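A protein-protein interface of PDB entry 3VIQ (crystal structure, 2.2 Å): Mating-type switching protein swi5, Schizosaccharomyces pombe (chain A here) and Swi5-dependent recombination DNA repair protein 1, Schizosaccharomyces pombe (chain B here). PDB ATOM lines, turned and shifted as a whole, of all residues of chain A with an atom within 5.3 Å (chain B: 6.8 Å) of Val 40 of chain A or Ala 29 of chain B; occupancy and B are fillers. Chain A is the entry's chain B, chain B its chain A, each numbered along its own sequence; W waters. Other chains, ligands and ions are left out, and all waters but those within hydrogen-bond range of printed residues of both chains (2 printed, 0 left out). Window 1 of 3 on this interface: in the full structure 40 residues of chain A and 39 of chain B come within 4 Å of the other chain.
Among the printed residues, pairs that only touch across the chains: Leu 31 of chain A with Ala 26 of chain B (3.8 Å), Leu 31 of chain A with Ala 29 of chain B (3.7 Å), Leu 31 of chain A with Arg 30 of chain B (3.3 Å), Leu 31 of chain A with Glu 33 of chain B (3.4 Å), Ala 36 of chain A with Thr 25 of chain B (3.8 Å), Ala 36 of chain A with Ala 26 of chain B (3.8 Å), Ala 36 of chain A with Ala 29 of chain B (3.6 Å), Lys 37 of chain A with Thr 25 of chain B (3.8 Å), Thr 39 of chain A with Val 32 of chain B (3.9 Å), Val 40 of chain A with Thr 25 of chain B (3.6 Å), Val 40 of chain A with Ala 29 of chain B (3.6 Å) and His 43 of chain A with Val 32 of chain B (3.6 Å).
Of the printed residues of chain B, Lys 37 of chain A touches Thr 25. Of chain B, only Thr 25 (3.6 Å) and Ala 29 (3.6 Å) come within 4 Å of Val 40 of chain A. Of the printed residues of chain B, His 43 of chain A touches Val 32 (3.6 Å). Ala 29 of chain B touches three residues of chain A. Ala 34 of chain B touches none of the printed residues of chain A. The nearest printed residue of chain B that does not touch His 43 of chain A is Thr 28 of chain B (6.6 Å).
Of the 11 printed residues of chain B, 6 touch a printed residue of chain A. Of the 11 printed residues of chain A, 6 touch a printed residue of chain B. Hydrophobic or aromatic side chains of chain A that line the printed part of chain B: Leu 31, Ala 36, Val 40 and His 43. Among the printed residues, 12 pairs touch across the chains. Among the printed residues, no Asp or Glu carboxylate lies within 4 Å of a Lys or Arg side-chain nitrogen of the other chain.
Water W1 lies within hydrogen-bond range of the side-chain hydroxyl of Thr 25 of chain B and the side-chain amino group of Lys 37 of chain A. Water W2 lies within hydrogen-bond range of the side-chain hydroxyl (OG1) of Thr 39 of chain A (2.6 Å) and the side-chain carboxylate (OE2) of Glu 33 of chain B (2.7 Å).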
ATOM      1  N   LEU A  31      -4.269  36.174 -19.964  1.00  0.00           N
ATOM      2  CA  LEU A  31      -3.335  35.066 -20.059  1.00  0.00           C
ATOM      3  C   LEU A  31      -2.185  35.380 -21.002  1.00  0.00           C
ATOM      4  O   LEU A  31      -2.387  35.969 -22.061  1.00  0.00           O
ATOM      5  CB  LEU A  31      -4.060  33.819 -20.560  1.00  0.00           C
ATOM      6  CG  LEU A  31      -5.234  33.272 -19.750  1.00  0.00           C
ATOM      7  CD1 LEU A  31      -5.764  31.989 -20.395  1.00  0.00           C
ATOM      8  CD2 LEU A  31      -4.843  33.025 -18.299  1.00  0.00           C
ATOM      9  N   ALA A  36      -5.708  28.147 -23.034  1.00  0.00           N
ATOM     10  CA  ALA A  36      -5.823  27.866 -21.609  1.00  0.00           C
ATOM     11  C   ALA A  36      -5.867  26.382 -21.325  1.00  0.00           C
ATOM     12  O   ALA A  36      -5.423  25.936 -20.271  1.00  0.00           O
ATOM     13  CB  ALA A  36      -7.074  28.540 -21.020  1.00  0.00           C
ATOM     14  N   LYS A  37      -6.444  25.617 -22.243  1.00  0.00           N
ATOM     15  CA  LYS A  37      -6.586  24.166 -22.057  1.00  0.00           C
ATOM     16  C   LYS A  37      -5.226  23.463 -22.049  1.00  0.00           C
ATOM     17  O   LYS A  37      -4.985  22.570 -21.268  1.00  0.00           O
ATOM     18  CB  LYS A  37      -7.465  23.607 -23.173  1.00  0.00           C
ATOM     19  CG  LYS A  37      -7.950  22.192 -23.002  1.00  0.00           C
ATOM     20  CD  LYS A  37      -8.966  21.851 -24.128  1.00  0.00           C
ATOM     21  CE  LYS A  37     -10.134  21.010 -23.626  1.00  0.00           C
ATOM     22  NZ  LYS A  37     -10.879  21.695 -22.530  1.00  0.00           N
ATOM     23  N   GLN A  38      -4.328  23.892 -22.920  1.00  0.00           N
ATOM     24  CA  GLN A  38      -2.970  23.365 -22.954  1.00  0.00           C
ATOM     25  C   GLN A  38      -2.238  23.715 -21.641  1.00  0.00           C
ATOM     26  O   GLN A  38      -1.593  22.865 -21.054  1.00  0.00           O
ATOM     27  CB  GLN A  38      -2.248  23.940 -24.183  1.00  0.00           C
ATOM     28  CG  GLN A  38      -0.731  23.725 -24.298  1.00  0.00           C
ATOM     29  CD  GLN A  38      -0.151  24.547 -25.458  1.00  0.00           C
ATOM     30  OE1 GLN A  38      -0.274  25.780 -25.489  1.00  0.00           O
ATOM     31  NE2 GLN A  38       0.456  23.866 -26.426  1.00  0.00           N
ATOM     32  N   THR A  39      -2.347  24.963 -21.198  1.00  0.00           N
ATOM     33  CA  THR A  39      -1.682  25.431 -19.973  1.00  0.00           C
ATOM     34  C   THR A  39      -2.090  24.595 -18.781  1.00  0.00           C
ATOM     35  O   THR A  39      -1.248  24.100 -18.047  1.00  0.00           O
ATOM     36  CB  THR A  39      -2.065  26.879 -19.676  1.00  0.00           C
ATOM     37  OG1 THR A  39      -1.571  27.685 -20.737  1.00  0.00           O
ATOM     38  CG2 THR A  39      -1.491  27.355 -18.344  1.00  0.00           C
ATOM     39  N   VAL A  40      -3.394  24.425 -18.619  1.00  0.00           N
ATOM     40  CA  VAL A  40      -3.942  23.703 -17.475  1.00  0.00           C
ATOM     41  C   VAL A  40      -3.600  22.220 -17.561  1.00  0.00           C
ATOM     42  O   VAL A  40      -3.185  21.627 -16.571  1.00  0.00           O
ATOM     43  CB  VAL A  40      -5.455  23.855 -17.381  1.00  0.00           C
ATOM     44  CG1 VAL A  40      -5.993  23.008 -16.245  1.00  0.00           C
ATOM     45  CG2 VAL A  40      -5.816  25.378 -17.228  1.00  0.00           C
ATOM     46  N   GLN A  41      -3.766  21.624 -18.740  1.00  0.00           N
ATOM     47  CA  GLN A  41      -3.429  20.203 -18.913  1.00  0.00           C
ATOM     48  C   GLN A  41      -1.927  19.967 -18.676  1.00  0.00           C
ATOM     49  O   GLN A  41      -1.547  19.009 -18.006  1.00  0.00           O
ATOM     50  CB  GLN A  41      -3.836  19.693 -20.311  1.00  0.00           C
ATOM     51  CG  GLN A  41      -3.759  18.177 -20.487  1.00  0.00           C
ATOM     52  CD  GLN A  41      -4.692  17.425 -19.512  1.00  0.00           C
ATOM     53  OE1 GLN A  41      -5.846  17.828 -19.299  1.00  0.00           O
ATOM     54  NE2 GLN A  41      -4.182  16.342 -18.914  1.00  0.00           N
ATOM     55  N   LYS A  42      -1.060  20.822 -19.204  1.00  0.00           N
ATOM     56  CA  LYS A  42       0.380  20.560 -19.013  1.00  0.00           C
ATOM     57  C   LYS A  42       0.711  20.570 -17.514  1.00  0.00           C
ATOM     58  O   LYS A  42       1.494  19.749 -17.043  1.00  0.00           O
ATOM     59  CB  LYS A  42       1.248  21.565 -19.765  1.00  0.00           C
ATOM     60  CG  LYS A  42       2.721  21.520 -19.420  1.00  0.00           C
ATOM     61  CD  LYS A  42       3.606  22.351 -20.392  1.00  0.00           C
ATOM     62  CE  LYS A  42       4.959  22.659 -19.733  1.00  0.00           C
ATOM     63  NZ  LYS A  42       6.080  22.846 -20.701  1.00  0.00           N
ATOM     64  N   HIS A  43       0.072  21.469 -16.770  1.00  0.00           N
ATOM     65  CA  HIS A  43       0.311  21.624 -15.344  1.00  0.00           C
ATOM     66  C   HIS A  43      -0.198  20.398 -14.620  1.00  0.00           C
ATOM     67  O   HIS A  43       0.528  19.819 -13.824  1.00  0.00           O
ATOM     68  CB  HIS A  43      -0.319  22.923 -14.778  1.00  0.00           C
ATOM     69  CG  HIS A  43      -0.059  23.131 -13.311  1.00  0.00           C
ATOM     70  ND1 HIS A  43      -1.048  23.035 -12.353  1.00  0.00           N
ATOM     71  CD2 HIS A  43       1.083  23.424 -12.643  1.00  0.00           C
ATOM     72  CE1 HIS A  43      -0.522  23.251 -11.161  1.00  0.00           C
ATOM     73  NE2 HIS A  43       0.773  23.471 -11.310  1.00  0.00           N
ATOM     74  N   ILE A  44      -1.413  19.981 -14.938  1.00  0.00           N
ATOM     75  CA  ILE A  44      -2.023  18.792 -14.303  1.00  0.00           C
ATOM     76  C   ILE A  44      -1.150  17.535 -14.491  1.00  0.00           C
ATOM     77  O   ILE A  44      -1.039  16.740 -13.591  1.00  0.00           O
ATOM     78  CB  ILE A  44      -3.434  18.520 -14.861  1.00  0.00           C
ATOM     79  CG1 ILE A  44      -4.432  19.504 -14.256  1.00  0.00           C
ATOM     80  CG2 ILE A  44      -3.928  17.053 -14.589  1.00  0.00           C
ATOM     81  CD1 ILE A  44      -5.841  19.294 -14.761  1.00  0.00           C
ATOM     82  N   ASP A  45      -0.550  17.358 -15.665  1.00  0.00           N
ATOM     83  CA  ASP A  45       0.244  16.156 -15.948  1.00  0.00           C
ATOM     84  C   ASP A  45       1.600  16.206 -15.176  1.00  0.00           C
ATOM     85  O   ASP A  45       2.054  15.209 -14.622  1.00  0.00           O
ATOM     86  CB  ASP A  45       0.512  16.036 -17.453  1.00  0.00           C
ATOM     87  CG  ASP A  45      -0.767  15.894 -18.293  1.00  0.00           C
ATOM     88  OD1 ASP A  45      -1.842  15.530 -17.759  1.00  0.00           O
ATOM     89  OD2 ASP A  45      -0.691  16.147 -19.516  1.00  0.00           O
ATOM     90  N   ILE B  24     -14.177  28.499 -16.898  1.00  0.00           N
ATOM     91  CA  ILE B  24     -13.453  27.904 -15.756  1.00  0.00           C
ATOM     92  C   ILE B  24     -12.016  27.567 -16.145  1.00  0.00           C
ATOM     93  O   ILE B  24     -11.051  27.887 -15.426  1.00  0.00           O
ATOM     94  CB  ILE B  24     -14.158  26.636 -15.221  1.00  0.00           C
ATOM     95  CG1 ILE B  24     -15.231  27.045 -14.200  1.00  0.00           C
ATOM     96  CG2 ILE B  24     -13.114  25.615 -14.585  1.00  0.00           C
ATOM     97  CD1 ILE B  24     -16.360  26.069 -14.123  1.00  0.00           C
ATOM     98  N   THR B  25     -11.873  26.964 -17.305  1.00  0.00           N
ATOM     99  CA  THR B  25     -10.559  26.633 -17.796  1.00  0.00           C
ATOM    100  C   THR B  25      -9.659  27.873 -17.922  1.00  0.00           C
ATOM    101  O   THR B  25      -8.469  27.826 -17.566  1.00  0.00           O
ATOM    102  CB  THR B  25     -10.683  25.887 -19.127  1.00  0.00           C
ATOM    103  OG1 THR B  25     -11.440  24.686 -18.903  1.00  0.00           O
ATOM    104  CG2 THR B  25      -9.306  25.559 -19.723  1.00  0.00           C
ATOM    105  N   ALA B  26     -10.219  28.982 -18.398  1.00  0.00           N
ATOM    106  CA  ALA B  26      -9.447  30.214 -18.574  1.00  0.00           C
ATOM    107  C   ALA B  26      -9.099  30.849 -17.217  1.00  0.00           C
ATOM    108  O   ALA B  26      -8.021  31.457 -17.049  1.00  0.00           O
ATOM    109  CB  ALA B  26     -10.186  31.189 -19.467  1.00  0.00           C
ATOM    110  N   GLU B  27      -9.988  30.679 -16.241  1.00  0.00           N
ATOM    111  CA  GLU B  27      -9.697  31.112 -14.879  1.00  0.00           C
ATOM    112  C   GLU B  27      -8.611  30.258 -14.216  1.00  0.00           C
ATOM    113  O   GLU B  27      -7.730  30.774 -13.533  1.00  0.00           O
ATOM    114  CB  GLU B  27     -10.974  31.128 -14.064  1.00  0.00           C
ATOM    115  CG  GLU B  27     -11.884  32.285 -14.511  1.00  0.00           C
ATOM    116  CD  GLU B  27     -13.328  32.154 -14.041  1.00  0.00           C
ATOM    117  OE1 GLU B  27     -13.798  31.010 -13.678  1.00  0.00           O
ATOM    118  OE2 GLU B  27     -13.987  33.221 -14.070  1.00  0.00           O
ATOM    119  N   THR B  28      -8.648  28.958 -14.442  1.00  0.00           N
ATOM    120  CA  THR B  28      -7.638  28.102 -13.877  1.00  0.00           C
ATOM    121  C   THR B  28      -6.281  28.415 -14.499  1.00  0.00           C
ATOM    122  O   THR B  28      -5.283  28.488 -13.778  1.00  0.00           O
ATOM    123  CB  THR B  28      -7.989  26.653 -14.065  1.00  0.00           C
ATOM    124  OG1 THR B  28      -9.293  26.439 -13.526  1.00  0.00           O
ATOM    125  CG2 THR B  28      -6.959  25.714 -13.353  1.00  0.00           C
ATOM    126  N   ALA B  29      -6.256  28.651 -15.816  1.00  0.00           N
ATOM    127  CA  ALA B  29      -5.022  28.966 -16.506  1.00  0.00           C
ATOM    128  C   ALA B  29      -4.380  30.205 -15.904  1.00  0.00           C
ATOM    129  O   ALA B  29      -3.160  30.220 -15.710  1.00  0.00           O
ATOM    130  CB  ALA B  29      -5.246  29.134 -18.026  1.00  0.00           C
ATOM    131  N   ARG B  30      -5.187  31.223 -15.580  1.00  0.00           N
ATOM    132  CA  ARG B  30      -4.657  32.446 -14.966  1.00  0.00           C
ATOM    133  C   ARG B  30      -3.908  32.131 -13.670  1.00  0.00           C
ATOM    134  O   ARG B  30      -2.849  32.671 -13.432  1.00  0.00           O
ATOM    135  CB  ARG B  30      -5.756  33.478 -14.690  1.00  0.00           C
ATOM    136  CG  ARG B  30      -5.227  34.818 -14.174  1.00  0.00           C
ATOM    137  CD  ARG B  30      -6.329  35.720 -13.612  1.00  0.00           C
ATOM    138  NE  ARG B  30      -6.943  35.156 -12.414  1.00  0.00           N
ATOM    139  CZ  ARG B  30      -6.337  35.056 -11.235  1.00  0.00           C
ATOM    140  NH1 ARG B  30      -5.087  35.478 -11.083  1.00  0.00           N
ATOM    141  NH2 ARG B  30      -6.985  34.523 -10.208  1.00  0.00           N
ATOM    142  N   LYS B  31      -4.471  31.257 -12.837  1.00  0.00           N
ATOM    143  CA  LYS B  31      -3.817  30.868 -11.588  1.00  0.00           C
ATOM    144  C   LYS B  31      -2.576  30.026 -11.872  1.00  0.00           C
ATOM    145  O   LYS B  31      -1.552  30.242 -11.272  1.00  0.00           O
ATOM    146  CB  LYS B  31      -4.770  30.105 -10.676  1.00  0.00           C
ATOM    147  CG  LYS B  31      -5.809  31.025 -10.049  1.00  0.00           C
ATOM    148  CD  LYS B  31      -7.043  30.297  -9.556  1.00  0.00           C
ATOM    149  CE  LYS B  31      -6.703  29.253  -8.481  1.00  0.00           C
ATOM    150  NZ  LYS B  31      -7.803  28.232  -8.361  1.00  0.00           N
ATOM    151  N   VAL B  32      -2.659  29.096 -12.815  1.00  0.00           N
ATOM    152  CA  VAL B  32      -1.489  28.303 -13.152  1.00  0.00           C
ATOM    153  C   VAL B  32      -0.337  29.191 -13.619  1.00  0.00           C
ATOM    154  O   VAL B  32       0.795  28.989 -13.176  1.00  0.00           O
ATOM    155  CB  VAL B  32      -1.789  27.179 -14.165  1.00  0.00           C
ATOM    156  CG1 VAL B  32      -0.486  26.520 -14.659  1.00  0.00           C
ATOM    157  CG2 VAL B  32      -2.724  26.164 -13.537  1.00  0.00           C
ATOM    158  N   GLU B  33      -0.624  30.183 -14.463  1.00  0.00           N
ATOM    159  CA  GLU B  33       0.395  31.128 -14.898  1.00  0.00           C
ATOM    160  C   GLU B  33       0.979  31.953 -13.727  1.00  0.00           C
ATOM    161  O   GLU B  33       2.185  32.197 -13.670  1.00  0.00           O
ATOM    162  CB  GLU B  33      -0.124  32.049 -16.026  1.00  0.00           C
ATOM    163  CG  GLU B  33      -0.217  31.329 -17.406  1.00  0.00           C
ATOM    164  CD  GLU B  33      -0.625  32.228 -18.563  1.00  0.00           C
ATOM    165  OE1 GLU B  33      -0.813  33.448 -18.360  1.00  0.00           O
ATOM    166  OE2 GLU B  33      -0.771  31.715 -19.700  1.00  0.00           O
ATOM    167  N   ALA B  34       0.132  32.368 -12.800  1.00  0.00           N
ATOM    168  CA  ALA B  34       0.587  33.138 -11.640  1.00  0.00           C
ATOM    169  C   ALA B  34       1.531  32.306 -10.744  1.00  0.00           C
ATOM    170  O   ALA B  34       2.558  32.795 -10.324  1.00  0.00           O
ATOM    171  CB  ALA B  34      -0.616  33.673 -10.828  1.00  0.00           C
HETATM  172  O   HOH W   1     -12.054  24.163 -21.320  1.00  0.00           O
HETATM  173  O   HOH W   2      -2.688  29.949 -20.274  1.00  0.00           O
